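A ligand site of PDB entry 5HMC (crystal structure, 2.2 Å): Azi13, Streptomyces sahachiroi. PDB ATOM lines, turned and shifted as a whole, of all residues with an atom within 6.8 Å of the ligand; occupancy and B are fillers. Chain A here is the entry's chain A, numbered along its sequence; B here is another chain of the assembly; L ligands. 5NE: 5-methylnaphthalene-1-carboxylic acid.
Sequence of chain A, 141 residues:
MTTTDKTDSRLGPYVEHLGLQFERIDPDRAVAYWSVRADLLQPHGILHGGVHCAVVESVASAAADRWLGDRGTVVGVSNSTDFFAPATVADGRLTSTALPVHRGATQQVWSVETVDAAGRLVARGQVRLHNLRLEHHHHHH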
ATOM      1  N   ARG A  10      12.886  25.685  39.962  1.00  0.00           N
ATOM      2  CA  ARG A  10      13.503  26.138  38.723  1.00  0.00           C
ATOM      3  C   ARG A  10      12.877  25.461  37.512  1.00  0.00           C
ATOM      4  O   ARG A  10      13.583  25.036  36.600  1.00  0.00           O
ATOM      5  CB  ARG A  10      15.003  25.883  38.735  1.00  0.00           C
ATOM      6  N   LEU A  11      11.546  25.374  37.511  1.00  0.00           N
ATOM      7  CA  LEU A  11      10.817  24.730  36.435  1.00  0.00           C
ATOM      8  C   LEU A  11       9.919  25.682  35.660  1.00  0.00           C
ATOM      9  O   LEU A  11       9.295  25.252  34.686  1.00  0.00           O
ATOM     10  CB  LEU A  11       9.969  23.580  36.993  1.00  0.00           C
ATOM     11  CG  LEU A  11      10.830  22.368  37.335  1.00  0.00           C
ATOM     12  CD1 LEU A  11       9.961  21.310  37.957  1.00  0.00           C
ATOM     13  CD2 LEU A  11      11.533  21.849  36.077  1.00  0.00           C
ATOM     14  N   GLY A  12       9.858  26.939  36.051  1.00  0.00           N
ATOM     15  CA  GLY A  12       9.089  27.920  35.322  1.00  0.00           C
ATOM     16  C   GLY A  12       7.771  28.203  36.002  1.00  0.00           C
ATOM     17  O   GLY A  12       7.322  27.485  36.896  1.00  0.00           O
ATOM     18  N   VAL A  15       4.624  25.557  35.401  1.00  0.00           N
ATOM     19  CA  VAL A  15       4.646  24.369  36.241  1.00  0.00           C
ATOM     20  C   VAL A  15       4.106  24.688  37.628  1.00  0.00           C
ATOM     21  O   VAL A  15       3.319  23.913  38.195  1.00  0.00           O
ATOM     22  CB  VAL A  15       6.060  23.774  36.294  1.00  0.00           C
ATOM     23  CG1 VAL A  15       6.108  22.648  37.317  1.00  0.00           C
ATOM     24  CG2 VAL A  15       6.443  23.249  34.936  1.00  0.00           C
ATOM     25  N   ALA A  54      -0.200  19.056  29.748  1.00  0.00           N
ATOM     26  CA  ALA A  54       0.801  19.936  30.336  1.00  0.00           C
ATOM     27  C   ALA A  54       1.516  19.256  31.499  1.00  0.00           C
ATOM     28  O   ALA A  54       2.727  19.447  31.681  1.00  0.00           O
ATOM     29  CB  ALA A  54       0.142  21.242  30.798  1.00  0.00           C
ATOM     30  N   GLU A  57       3.888  16.891  29.861  1.00  0.00           N
ATOM     31  CA  GLU A  57       5.017  17.634  29.323  1.00  0.00           C
ATOM     32  C   GLU A  57       5.978  18.046  30.438  1.00  0.00           C
ATOM     33  O   GLU A  57       7.207  17.970  30.280  1.00  0.00           O
ATOM     34  CB  GLU A  57       4.520  18.863  28.565  1.00  0.00           C
ATOM     35  CG  GLU A  57       5.611  19.636  27.836  1.00  0.00           C
ATOM     36  CD  GLU A  57       5.832  19.113  26.432  1.00  0.00           C
ATOM     37  OE1 GLU A  57       4.946  18.365  25.953  1.00  0.00           O
ATOM     38  OE2 GLU A  57       6.864  19.453  25.822  1.00  0.00           O
ATOM     39  N   SER A  58       5.421  18.485  31.579  1.00  0.00           N
ATOM     40  CA  SER A  58       6.245  19.015  32.652  1.00  0.00           C
ATOM     41  C   SER A  58       7.142  17.936  33.248  1.00  0.00           C
ATOM     42  O   SER A  58       8.353  18.138  33.450  1.00  0.00           O
ATOM     43  CB  SER A  58       5.358  19.617  33.736  1.00  0.00           C
ATOM     44  OG  SER A  58       4.531  20.652  33.246  1.00  0.00           O
ATOM     45  N   VAL A  59       6.573  16.769  33.549  1.00  0.00           N
ATOM     46  CA  VAL A  59       7.312  15.756  34.286  1.00  0.00           C
ATOM     47  C   VAL A  59       8.346  15.111  33.376  1.00  0.00           C
ATOM     48  O   VAL A  59       9.459  14.787  33.814  1.00  0.00           O
ATOM     49  CB  VAL A  59       6.329  14.741  34.901  1.00  0.00           C
ATOM     50  CG1 VAL A  59       7.058  13.730  35.751  1.00  0.00           C
ATOM     51  CG2 VAL A  59       5.303  15.483  35.758  1.00  0.00           C
ATOM     52  N   SER A  61       9.821  16.594  30.603  1.00  0.00           N
ATOM     53  CA  SER A  61      10.879  17.544  30.248  1.00  0.00           C
ATOM     54  C   SER A  61      11.817  17.779  31.416  1.00  0.00           C
ATOM     55  O   SER A  61      13.026  17.950  31.224  1.00  0.00           O
ATOM     56  CB  SER A  61      10.286  18.882  29.798  1.00  0.00           C
ATOM     57  OG  SER A  61       9.565  18.746  28.594  1.00  0.00           O
ATOM     58  N   ALA A  62      11.281  17.814  32.639  1.00  0.00           N
ATOM     59  CA  ALA A  62      12.123  17.908  33.828  1.00  0.00           C
ATOM     60  C   ALA A  62      13.135  16.768  33.863  1.00  0.00           C
ATOM     61  O   ALA A  62      14.331  16.987  34.075  1.00  0.00           O
ATOM     62  CB  ALA A  62      11.267  17.890  35.088  1.00  0.00           C
ATOM     63  N   ASP A  65      15.641  17.095  30.868  1.00  0.00           N
ATOM     64  CA  ASP A  65      16.606  18.159  31.116  1.00  0.00           C
ATOM     65  C   ASP A  65      17.642  17.707  32.131  1.00  0.00           C
ATOM     66  O   ASP A  65      18.838  17.949  31.953  1.00  0.00           O
ATOM     67  CB  ASP A  65      15.861  19.392  31.609  1.00  0.00           C
ATOM     68  CG  ASP A  65      16.646  20.655  31.426  1.00  0.00           C
ATOM     69  OD1 ASP A  65      17.285  20.816  30.369  1.00  0.00           O
ATOM     70  OD2 ASP A  65      16.601  21.496  32.339  1.00  0.00           O
ATOM     71  N   THR A  73      20.812  21.394  26.551  1.00  0.00           N
ATOM     72  CA  THR A  73      19.440  21.635  26.989  1.00  0.00           C
ATOM     73  C   THR A  73      18.424  21.028  26.007  1.00  0.00           C
ATOM     74  O   THR A  73      18.744  20.756  24.844  1.00  0.00           O
ATOM     75  CB  THR A  73      19.193  23.131  27.150  1.00  0.00           C
ATOM     76  OG1 THR A  73      17.938  23.331  27.828  1.00  0.00           O
ATOM     77  CG2 THR A  73      19.198  23.833  25.788  1.00  0.00           C
ATOM     78  N   VAL A  74      17.192  20.842  26.489  1.00  0.00           N
ATOM     79  CA  VAL A  74      16.162  20.155  25.722  1.00  0.00           C
ATOM     80  C   VAL A  74      15.062  21.126  25.322  1.00  0.00           C
ATOM     81  O   VAL A  74      14.761  22.107  26.017  1.00  0.00           O
ATOM     82  CB  VAL A  74      15.560  18.958  26.510  1.00  0.00           C
ATOM     83  CG1 VAL A  74      16.662  18.115  27.098  1.00  0.00           C
ATOM     84  CG2 VAL A  74      14.618  19.444  27.596  1.00  0.00           C
ATOM     85  N   VAL A  75      14.436  20.847  24.180  1.00  0.00           N
ATOM     86  CA  VAL A  75      13.274  21.577  23.685  1.00  0.00           C
ATOM     87  C   VAL A  75      12.181  20.559  23.361  1.00  0.00           C
ATOM     88  O   VAL A  75      12.477  19.508  22.787  1.00  0.00           O
ATOM     89  CB  VAL A  75      13.626  22.435  22.444  1.00  0.00           C
ATOM     90  CG1 VAL A  75      14.398  21.603  21.454  1.00  0.00           C
ATOM     91  CG2 VAL A  75      12.377  22.985  21.779  1.00  0.00           C
ATOM     92  N   GLY A  76      10.941  20.856  23.751  1.00  0.00           N
ATOM     93  CA  GLY A  76       9.835  19.981  23.403  1.00  0.00           C
ATOM     94  C   GLY A  76       9.601  19.915  21.899  1.00  0.00           C
ATOM     95  O   GLY A  76       9.625  20.934  21.203  1.00  0.00           O
ATOM     96  N   VAL A  77       9.408  18.697  21.392  1.00  0.00           N
ATOM     97  CA  VAL A  77       9.125  18.435  19.989  1.00  0.00           C
ATOM     98  C   VAL A  77       7.669  18.003  19.771  1.00  0.00           C
ATOM     99  O   VAL A  77       7.004  18.501  18.855  1.00  0.00           O
ATOM    100  CB  VAL A  77      10.097  17.388  19.398  1.00  0.00           C
ATOM    101  CG1 VAL A  77       9.775  17.109  17.932  1.00  0.00           C
ATOM    102  CG2 VAL A  77      11.545  17.835  19.545  1.00  0.00           C
ATOM    103  N   VAL A 127       6.331  12.027  25.369  1.00  0.00           N
ATOM    104  CA  VAL A 127       6.884  13.324  25.005  1.00  0.00           C
ATOM    105  C   VAL A 127       8.209  13.084  24.279  1.00  0.00           C
ATOM    106  O   VAL A 127       9.077  12.362  24.780  1.00  0.00           O
ATOM    107  CB  VAL A 127       7.088  14.240  26.216  1.00  0.00           C
ATOM    108  CG1 VAL A 127       7.620  15.589  25.789  1.00  0.00           C
ATOM    109  CG2 VAL A 127       5.795  14.417  26.934  1.00  0.00           C
ATOM    110  N   LEU A 129      11.570  14.946  22.803  1.00  0.00           N
ATOM    111  CA  LEU A 129      12.364  16.137  23.023  1.00  0.00           C
ATOM    112  C   LEU A 129      13.605  16.102  22.135  1.00  0.00           C
ATOM    113  O   LEU A 129      14.108  15.043  21.774  1.00  0.00           O
ATOM    114  CB  LEU A 129      12.786  16.260  24.490  1.00  0.00           C
ATOM    115  CG  LEU A 129      11.607  16.290  25.461  1.00  0.00           C
ATOM    116  CD1 LEU A 129      11.523  15.010  26.307  1.00  0.00           C
ATOM    117  CD2 LEU A 129      11.647  17.534  26.336  1.00  0.00           C
ATOM    118  N   LEU B  41       5.335  30.389  30.559  1.00  0.00           N
ATOM    119  CA  LEU B  41       6.636  30.000  30.037  1.00  0.00           C
ATOM    120  C   LEU B  41       7.212  28.810  30.778  1.00  0.00           C
ATOM    121  O   LEU B  41       6.874  28.562  31.940  1.00  0.00           O
ATOM    122  CB  LEU B  41       7.623  31.160  30.138  1.00  0.00           C
ATOM    123  CG  LEU B  41       7.254  32.439  29.405  1.00  0.00           C
ATOM    124  CD1 LEU B  41       8.149  33.572  29.860  1.00  0.00           C
ATOM    125  CD2 LEU B  41       7.338  32.212  27.898  1.00  0.00           C
ATOM    126  N   GLN B  42       8.073  28.079  30.089  1.00  0.00           N
ATOM    127  CA  GLN B  42       8.943  27.099  30.730  1.00  0.00           C
ATOM    128  C   GLN B  42      10.284  27.782  31.041  1.00  0.00           C
ATOM    129  O   GLN B  42      10.465  28.953  30.700  1.00  0.00           O
ATOM    130  CB  GLN B  42       9.050  25.876  29.818  1.00  0.00           C
ATOM    131  CG  GLN B  42       9.414  26.129  28.367  1.00  0.00           C
ATOM    132  CD  GLN B  42      10.899  25.919  28.111  1.00  0.00           C
ATOM    133  OE1 GLN B  42      11.714  26.158  28.993  1.00  0.00           O
ATOM    134  NE2 GLN B  42      11.253  25.403  26.950  1.00  0.00           N
ATOM    135  N   PRO B  43      11.230  27.132  31.735  1.00  0.00           N
ATOM    136  CA  PRO B  43      12.353  27.887  32.328  1.00  0.00           C
ATOM    137  C   PRO B  43      13.288  28.589  31.347  1.00  0.00           C
ATOM    138  O   PRO B  43      14.051  29.469  31.769  1.00  0.00           O
ATOM    139  CB  PRO B  43      13.122  26.824  33.126  1.00  0.00           C
ATOM    140  CG  PRO B  43      12.193  25.733  33.334  1.00  0.00           C
ATOM    141  CD  PRO B  43      11.231  25.725  32.185  1.00  0.00           C
ATOM    142  N   HIS B  44      13.288  28.235  30.061  1.00  0.00           N
ATOM    143  CA  HIS B  44      14.149  28.878  29.088  1.00  0.00           C
ATOM    144  C   HIS B  44      13.444  29.987  28.315  1.00  0.00           C
ATOM    145  O   HIS B  44      13.856  30.329  27.203  1.00  0.00           O
ATOM    146  CB  HIS B  44      14.712  27.832  28.125  1.00  0.00           C
ATOM    147  CG  HIS B  44      15.314  26.659  28.810  1.00  0.00           C
ATOM    148  ND1 HIS B  44      15.078  25.356  28.420  1.00  0.00           N
ATOM    149  CD2 HIS B  44      16.149  26.584  29.876  1.00  0.00           C
ATOM    150  CE1 HIS B  44      15.740  24.531  29.220  1.00  0.00           C
ATOM    151  NE2 HIS B  44      16.393  25.256  30.115  1.00  0.00           N
ATOM    152  N   ILE B  46      10.604  30.338  26.695  1.00  0.00           N
ATOM    153  CA  ILE B  46       9.673  30.099  25.607  1.00  0.00           C
ATOM    154  C   ILE B  46       8.397  29.453  26.178  1.00  0.00           C
ATOM    155  O   ILE B  46       8.338  29.063  27.341  1.00  0.00           O
ATOM    156  CB  ILE B  46      10.267  29.237  24.486  1.00  0.00           C
ATOM    157  CG1 ILE B  46      10.682  27.870  25.018  1.00  0.00           C
ATOM    158  CG2 ILE B  46      11.484  29.913  23.891  1.00  0.00           C
ATOM    159  CD1 ILE B  46      11.216  26.955  23.933  1.00  0.00           C
ATOM    160  N   LEU B  47       7.380  29.375  25.331  1.00  0.00           N
ATOM    161  CA  LEU B  47       6.107  28.830  25.768  1.00  0.00           C
ATOM    162  C   LEU B  47       6.266  27.375  26.218  1.00  0.00           C
ATOM    163  O   LEU B  47       6.895  26.569  25.534  1.00  0.00           O
ATOM    164  CB  LEU B  47       5.093  28.910  24.628  1.00  0.00           C
ATOM    165  CG  LEU B  47       3.675  28.501  25.022  1.00  0.00           C
ATOM    166  CD1 LEU B  47       3.123  29.450  26.076  1.00  0.00           C
ATOM    167  CD2 LEU B  47       2.793  28.477  23.811  1.00  0.00           C
ATOM    168  N   HIS B  48       5.731  27.088  27.405  1.00  0.00           N
ATOM    169  CA  HIS B  48       5.586  25.713  27.885  1.00  0.00           C
ATOM    170  C   HIS B  48       4.777  24.904  26.871  1.00  0.00           C
ATOM    171  O   HIS B  48       3.724  25.356  26.420  1.00  0.00           O
ATOM    172  CB  HIS B  48       4.894  25.751  29.255  1.00  0.00           C
ATOM    173  CG  HIS B  48       4.904  24.458  30.007  1.00  0.00           C
ATOM    174  ND1 HIS B  48       4.269  23.325  29.551  1.00  0.00           N
ATOM    175  CD2 HIS B  48       5.423  24.135  31.212  1.00  0.00           C
ATOM    176  CE1 HIS B  48       4.420  22.348  30.439  1.00  0.00           C
ATOM    177  NE2 HIS B  48       5.125  22.809  31.446  1.00  0.00           N
ATOM    178  N   GLY B  49       5.304  23.754  26.465  1.00  0.00           N
ATOM    179  CA  GLY B  49       4.667  22.985  25.409  1.00  0.00           C
ATOM    180  C   GLY B  49       3.260  22.537  25.785  1.00  0.00           C
ATOM    181  O   GLY B  49       2.368  22.474  24.947  1.00  0.00           O
ATOM    182  N   GLY B  50       3.047  22.245  27.064  1.00  0.00           N
ATOM    183  CA  GLY B  50       1.716  21.905  27.528  1.00  0.00           C
ATOM    184  C   GLY B  50       0.685  22.969  27.210  1.00  0.00           C
ATOM    185  O   GLY B  50      -0.500  22.662  27.057  1.00  0.00           O
ATOM    186  N   VAL B  51       1.114  24.232  27.084  1.00  0.00           N
ATOM    187  CA  VAL B  51       0.149  25.289  26.756  1.00  0.00           C
ATOM    188  C   VAL B  51      -0.379  25.096  25.333  1.00  0.00           C
ATOM    189  O   VAL B  51      -1.586  25.245  25.082  1.00  0.00           O
ATOM    190  CB  VAL B  51       0.783  26.676  26.960  1.00  0.00           C
ATOM    191  CG1 VAL B  51      -0.196  27.775  26.527  1.00  0.00           C
ATOM    192  CG2 VAL B  51       1.170  26.860  28.416  1.00  0.00           C
ATOM    193  N   PHE B  83       5.097  20.621  18.163  1.00  0.00           N
ATOM    194  CA  PHE B  83       5.589  21.985  18.321  1.00  0.00           C
ATOM    195  C   PHE B  83       6.656  22.251  17.265  1.00  0.00           C
ATOM    196  O   PHE B  83       7.705  21.594  17.271  1.00  0.00           O
ATOM    197  CB  PHE B  83       6.161  22.225  19.721  1.00  0.00           C
ATOM    198  CG  PHE B  83       5.440  21.501  20.813  1.00  0.00           C
ATOM    199  CD1 PHE B  83       4.098  21.776  21.089  1.00  0.00           C
ATOM    200  CD2 PHE B  83       6.098  20.557  21.596  1.00  0.00           C
ATOM    201  CE1 PHE B  83       3.425  21.120  22.115  1.00  0.00           C
ATOM    202  CE2 PHE B  83       5.430  19.881  22.612  1.00  0.00           C
ATOM    203  CZ  PHE B  83       4.084  20.165  22.878  1.00  0.00           C
HETATM  204  O1N 5NE L   1       8.703  21.100  27.006  1.00  0.00           O
HETATM  205  C1L 5NE L   1       8.359  22.096  27.675  1.00  0.00           C
HETATM  206  O1M 5NE L   1       7.573  22.957  27.238  1.00  0.00           O
HETATM  207  C1J 5NE L   1       8.903  22.197  29.064  1.00  0.00           C
HETATM  208  C1E 5NE L   1      10.360  22.214  29.298  1.00  0.00           C
HETATM  209  C1F 5NE L   1      11.309  22.172  28.284  1.00  0.00           C
HETATM  210  C1A 5NE L   1      12.674  22.191  28.603  1.00  0.00           C
HETATM  211  C1I 5NE L   1       8.039  22.231  30.157  1.00  0.00           C
HETATM  212  C1H 5NE L   1       8.520  22.284  31.470  1.00  0.00           C
HETATM  213  C1G 5NE L   1       9.885  22.312  31.747  1.00  0.00           C
HETATM  214  C1D 5NE L   1      10.794  22.275  30.709  1.00  0.00           C
HETATM  215  C1C 5NE L   1      12.231  22.288  30.997  1.00  0.00           C
HETATM  216  C1O 5NE L   1      12.650  22.345  32.441  1.00  0.00           C
HETATM  217  C1B 5NE L   1      13.130  22.256  29.919  1.00  0.00           C
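O of Glu 57 sits at hydrogen-bond distance from OG of Ser 61 (3.0 Å).
OG of Ser 58 is in hydrogen-bond range of NE2 of His 48 of chain B (2.9 Å).
ND1 of His 48 of chain B lies within hydrogen-bond range of N of Gly 50 of chain B, at 3.0 Å.
N of His 44 of chain B is in hydrogen-bond range of OE1 of Gln 42 of chain B, at 2.8 Å.
NE2 of His 44 of chain B sits close to OG1 of Thr 73, at 3.4 Å.
The backbone NH (N) of Gly 49 of chain B lies within hydrogen-bond range of an oxygen (O1M) of the ligand (2.5 Å).
The side-chain carboxylate (OE2) of Glu 57 sits close to an oxygen (O1N) of the ligand (2.7 Å).
An oxygen (O1N) of the ligand lies within hydrogen-bond range of the side-chain hydroxyl (OG) of Ser 61, at 3.0 Å.
Leu 11 touches the ligand (CD2 to C1O, 3.8 Å).
Val 74 touches the ligand (O to C1A, 3.3 Å).
Gly 76 touches the ligand (CA to O1N, 3.9 Å).
NE2 of Gln 42 of chain B touches C1F of the ligand (3.5 Å).
Pro 43 of chain B touches the ligand.
His 44 of chain B touches the ligand.
NE2 of His 48 of chain B touches C1I of the ligand, at 3.2 Å.
Ten residues have an atom within 4 Å of the ligand: Leu 11, Glu 57, Ser 61, Val 74, Gly 76, Gln 42 of chain B, Pro 43 of chain B, His 44 of chain B, His 48 of chain B and Gly 49 of chain B.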
